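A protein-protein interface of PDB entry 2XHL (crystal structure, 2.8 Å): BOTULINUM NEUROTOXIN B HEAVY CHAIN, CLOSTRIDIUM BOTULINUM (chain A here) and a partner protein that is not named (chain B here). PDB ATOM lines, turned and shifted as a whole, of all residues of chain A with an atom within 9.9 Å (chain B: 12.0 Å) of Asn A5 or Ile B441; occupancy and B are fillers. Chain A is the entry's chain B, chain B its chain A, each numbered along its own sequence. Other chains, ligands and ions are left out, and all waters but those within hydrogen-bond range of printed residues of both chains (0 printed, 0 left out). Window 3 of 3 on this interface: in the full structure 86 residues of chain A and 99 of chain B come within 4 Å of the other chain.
SG of Cys B437 forms a disulfide with SG of Cys A8, 2.0 Å away.
The backbone NH of Val B438 lies within hydrogen-bond range of the backbone carbonyl oxygen of Gln A7, at 3.1 Å.
The side-chain carboxylate (OD1) of Asp A95 sits close to the backbone carbonyl oxygen (O) of Val B438 (3.0 Å).
O of Asn A5 touches CB of Ile B441 (3.3 Å).
Gln A7 touches Met B436.
O of Gln A7 touches CA of Cys B437 (3.4 Å).
CB of Cys A8 touches CG of Gln B435 (3.7 Å).
Met B436 touches Cys A8 (O to CA, 3.4 Å).
OE1 of Gln B435 touches CE of Lys A91, at 3.4 Å.
O of Cys B437 touches CA of Phe A93 (3.3 Å).
CD2 of Phe A93 touches CA of Asp B439, at 3.9 Å.
Asp A95 touches Asp B439 (OD2 to OD2, 3.9 Å).
Of the 8 printed residues of chain A, 6 touch a printed residue of chain B.
Printed residues of chain A that touch a printed residue of chain B: Asn A5, Gln A7, Cys A8, Lys A91, Phe A93 and Asp A95.
Hydrophobic or aromatic side chains of chain A within 4 Å of the printed part of chain B: Phe A93.
Printed residues of chain B that touch a printed residue of chain A: Gln B435, Met B436, Cys B437, Val B438, Asp B439 and Ile B441.
Among the printed residues, 12 pairs touch across the chains.
Asn A5 touches just one residue of chain B: Ile B441.
No residue of chain B comes within 4 Å of Leu A6.
Gln A7 touches three residues of chain B.
Of the printed residues of chain B, Cys A8 touches Gln B435 (3.7 Å), Met B436 (3.4 Å) and Cys B437 (2.0 Å).
Of the printed residues of chain B, Lys A91 touches Gln B435.
Leu A126 touches none of the printed residues of chain B.
Printed residues of chain A within 4 Å of Met B436: Gln A7 (3.9 Å) and Cys A8 (3.4 Å).
Of the printed residues of chain A, Asp B439 touches Phe A93 and Asp A95.
Of chain A, only Asn A5 (3.3 Å) comes within 4 Å of Ile B441.
The nearest residue of chain B that does not touch Asn A5 is Gly B440 (4.2 Å).
The nearest printed residue of chain A that does not touch Met B436 is Phe A93 (5.6 Å).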
ATOM      1  N   ASN A   5      10.753 -29.789  16.177  1.00  0.00           N
ATOM      2  CA  ASN A   5      11.994 -29.762  15.346  1.00  0.00           C
ATOM      3  C   ASN A   5      11.769 -29.112  13.985  1.00  0.00           C
ATOM      4  O   ASN A   5      10.680 -29.210  13.416  1.00  0.00           O
ATOM      5  CB  ASN A   5      12.547 -31.179  15.155  1.00  0.00           C
ATOM      6  CG  ASN A   5      12.712 -31.928  16.468  1.00  0.00           C
ATOM      7  OD1 ASN A   5      13.058 -31.343  17.498  1.00  0.00           O
ATOM      8  ND2 ASN A   5      12.466 -33.233  16.434  1.00  0.00           N
ATOM      9  N   LEU A   6      12.804 -28.452  13.469  1.00  0.00           N
ATOM     10  CA  LEU A   6      12.754 -27.847  12.138  1.00  0.00           C
ATOM     11  C   LEU A   6      13.022 -28.875  11.042  1.00  0.00           C
ATOM     12  O   LEU A   6      13.900 -29.733  11.176  1.00  0.00           O
ATOM     13  CB  LEU A   6      13.750 -26.686  12.023  1.00  0.00           C
ATOM     14  CG  LEU A   6      13.389 -25.352  12.684  1.00  0.00           C
ATOM     15  CD1 LEU A   6      14.642 -24.526  12.934  1.00  0.00           C
ATOM     16  CD2 LEU A   6      12.379 -24.567  11.847  1.00  0.00           C
ATOM     17  N   GLN A   7      12.251 -28.777   9.963  1.00  0.00           N
ATOM     18  CA  GLN A   7      12.414 -29.639   8.800  1.00  0.00           C
ATOM     19  C   GLN A   7      13.058 -28.831   7.672  1.00  0.00           C
ATOM     20  O   GLN A   7      12.365 -28.201   6.870  1.00  0.00           O
ATOM     21  CB  GLN A   7      11.056 -30.206   8.372  1.00  0.00           C
ATOM     22  CG  GLN A   7      11.117 -31.292   7.302  1.00  0.00           C
ATOM     23  CD  GLN A   7       9.743 -31.821   6.914  1.00  0.00           C
ATOM     24  OE1 GLN A   7       8.846 -31.944   7.756  1.00  0.00           O
ATOM     25  NE2 GLN A   7       9.577 -32.143   5.633  1.00  0.00           N
ATOM     26  N   CYS A   8      14.389 -28.848   7.626  1.00  0.00           N
ATOM     27  CA  CYS A   8      15.136 -28.028   6.675  1.00  0.00           C
ATOM     28  C   CYS A   8      15.888 -28.848   5.626  1.00  0.00           C
ATOM     29  O   CYS A   8      16.638 -29.770   5.956  1.00  0.00           O
ATOM     30  CB  CYS A   8      16.102 -27.086   7.406  1.00  0.00           C
ATOM     31  SG  CYS A   8      15.332 -26.022   8.656  1.00  0.00           S
ATOM     32  N   LYS A  91      19.043 -18.917   6.374  1.00  0.00           N
ATOM     33  CA  LYS A  91      17.829 -19.643   6.719  1.00  0.00           C
ATOM     34  C   LYS A  91      16.613 -18.989   6.059  1.00  0.00           C
ATOM     35  O   LYS A  91      16.420 -17.776   6.177  1.00  0.00           O
ATOM     36  CB  LYS A  91      17.665 -19.644   8.239  1.00  0.00           C
ATOM     37  CG  LYS A  91      17.149 -20.938   8.835  1.00  0.00           C
ATOM     38  CD  LYS A  91      17.218 -20.873  10.354  1.00  0.00           C
ATOM     39  CE  LYS A  91      16.998 -22.233  10.978  1.00  0.00           C
ATOM     40  NZ  LYS A  91      17.164 -22.190  12.457  1.00  0.00           N
ATOM     41  N   PHE A  93      12.169 -19.753   4.885  1.00  0.00           N
ATOM     42  CA  PHE A  93      10.960 -20.479   5.267  1.00  0.00           C
ATOM     43  C   PHE A  93       9.913 -20.460   4.162  1.00  0.00           C
ATOM     44  O   PHE A  93       9.453 -19.393   3.755  1.00  0.00           O
ATOM     45  CB  PHE A  93      10.374 -19.887   6.553  1.00  0.00           C
ATOM     46  CG  PHE A  93      11.303 -19.954   7.730  1.00  0.00           C
ATOM     47  CD1 PHE A  93      12.206 -18.925   7.981  1.00  0.00           C
ATOM     48  CD2 PHE A  93      11.279 -21.048   8.589  1.00  0.00           C
ATOM     49  CE1 PHE A  93      13.076 -18.986   9.067  1.00  0.00           C
ATOM     50  CE2 PHE A  93      12.141 -21.116   9.681  1.00  0.00           C
ATOM     51  CZ  PHE A  93      13.041 -20.081   9.920  1.00  0.00           C
ATOM     52  N   ASP A  95       6.448 -22.998   2.343  1.00  0.00           N
ATOM     53  CA  ASP A  95       5.562 -24.159   2.298  1.00  0.00           C
ATOM     54  C   ASP A  95       5.499 -24.771   0.896  1.00  0.00           C
ATOM     55  O   ASP A  95       4.751 -25.723   0.661  1.00  0.00           O
ATOM     56  CB  ASP A  95       4.157 -23.771   2.768  1.00  0.00           C
ATOM     57  CG  ASP A  95       4.081 -23.538   4.268  1.00  0.00           C
ATOM     58  OD1 ASP A  95       4.279 -24.505   5.042  1.00  0.00           O
ATOM     59  OD2 ASP A  95       3.807 -22.386   4.673  1.00  0.00           O
ATOM     60  N   LEU A 126       8.659 -37.814   4.035  1.00  0.00           N
ATOM     61  CA  LEU A 126       8.468 -38.223   5.424  1.00  0.00           C
ATOM     62  C   LEU A 126       9.430 -39.343   5.832  1.00  0.00           C
ATOM     63  O   LEU A 126      10.362 -39.112   6.605  1.00  0.00           O
ATOM     64  CB  LEU A 126       7.007 -38.643   5.648  1.00  0.00           C
ATOM     65  CG  LEU A 126       6.424 -38.685   7.066  1.00  0.00           C
ATOM     66  CD1 LEU A 126       6.281 -37.282   7.649  1.00  0.00           C
ATOM     67  CD2 LEU A 126       5.073 -39.391   7.054  1.00  0.00           C
ATOM     68  N   GLN B 435      19.398 -22.671   3.530  1.00  0.00           N
ATOM     69  CA  GLN B 435      18.646 -23.592   4.374  1.00  0.00           C
ATOM     70  C   GLN B 435      17.150 -23.366   4.173  1.00  0.00           C
ATOM     71  O   GLN B 435      16.597 -22.365   4.632  1.00  0.00           O
ATOM     72  CB  GLN B 435      19.039 -23.404   5.842  1.00  0.00           C
ATOM     73  CG  GLN B 435      18.849 -24.639   6.708  1.00  0.00           C
ATOM     74  CD  GLN B 435      19.555 -24.528   8.048  1.00  0.00           C
ATOM     75  OE1 GLN B 435      19.271 -23.633   8.846  1.00  0.00           O
ATOM     76  NE2 GLN B 435      20.480 -25.446   8.304  1.00  0.00           N
ATOM     77  N   MET B 436      16.510 -24.299   3.473  1.00  0.00           N
ATOM     78  CA  MET B 436      15.092 -24.189   3.125  1.00  0.00           C
ATOM     79  C   MET B 436      14.212 -24.983   4.083  1.00  0.00           C
ATOM     80  O   MET B 436      14.128 -26.210   3.996  1.00  0.00           O
ATOM     81  CB  MET B 436      14.849 -24.653   1.686  1.00  0.00           C
ATOM     82  CG  MET B 436      15.545 -23.814   0.633  1.00  0.00           C
ATOM     83  SD  MET B 436      14.863 -24.076  -1.008  1.00  0.00           S
ATOM     84  CE  MET B 436      15.720 -22.799  -1.918  1.00  0.00           C
ATOM     85  N   CYS B 437      13.547 -24.270   4.985  1.00  0.00           N
ATOM     86  CA  CYS B 437      12.748 -24.907   6.024  1.00  0.00           C
ATOM     87  C   CYS B 437      11.249 -24.789   5.753  1.00  0.00           C
ATOM     88  O   CYS B 437      10.792 -23.815   5.149  1.00  0.00           O
ATOM     89  CB  CYS B 437      13.121 -24.338   7.395  1.00  0.00           C
ATOM     90  SG  CYS B 437      14.918 -24.282   7.681  1.00  0.00           S
ATOM     91  N   VAL B 438      10.496 -25.792   6.203  1.00  0.00           N
ATOM     92  CA  VAL B 438       9.061 -25.917   5.910  1.00  0.00           C
ATOM     93  C   VAL B 438       8.216 -24.790   6.522  1.00  0.00           C
ATOM     94  O   VAL B 438       7.144 -24.465   6.003  1.00  0.00           O
ATOM     95  CB  VAL B 438       8.514 -27.316   6.334  1.00  0.00           C
ATOM     96  CG1 VAL B 438       7.011 -27.430   6.090  1.00  0.00           C
ATOM     97  CG2 VAL B 438       9.240 -28.420   5.582  1.00  0.00           C
ATOM     98  N   ASP B 439       8.705 -24.197   7.607  1.00  0.00           N
ATOM     99  CA  ASP B 439       7.979 -23.136   8.302  1.00  0.00           C
ATOM    100  C   ASP B 439       6.974 -23.691   9.313  1.00  0.00           C
ATOM    101  O   ASP B 439       6.228 -22.941   9.941  1.00  0.00           O
ATOM    102  CB  ASP B 439       7.265 -22.230   7.296  1.00  0.00           C
ATOM    103  CG  ASP B 439       6.582 -21.049   7.956  1.00  0.00           C
ATOM    104  OD1 ASP B 439       6.785 -20.846   9.172  1.00  0.00           O
ATOM    105  OD2 ASP B 439       5.844 -20.321   7.260  1.00  0.00           O
ATOM    106  N   GLY B 440       6.970 -25.012   9.468  1.00  0.00           N
ATOM    107  CA  GLY B 440       6.113 -25.690  10.434  1.00  0.00           C
ATOM    108  C   GLY B 440       6.947 -26.387  11.492  1.00  0.00           C
ATOM    109  O   GLY B 440       8.176 -26.453  11.371  1.00  0.00           O
ATOM    110  N   ILE B 441       6.274 -26.905  12.526  1.00  0.00           N
ATOM    111  CA  ILE B 441       6.914 -27.614  13.651  1.00  0.00           C
ATOM    112  C   ILE B 441       8.076 -26.820  14.265  1.00  0.00           C
ATOM    113  O   ILE B 441       8.068 -25.584  14.290  1.00  0.00           O
ATOM    114  CB  ILE B 441       7.403 -29.047  13.257  1.00  0.00           C
ATOM    115  CG1 ILE B 441       6.402 -29.746  12.325  1.00  0.00           C
ATOM    116  CG2 ILE B 441       7.649 -29.897  14.513  1.00  0.00           C
ATOM    117  CD1 ILE B 441       7.020 -30.827  11.447  1.00  0.00           C
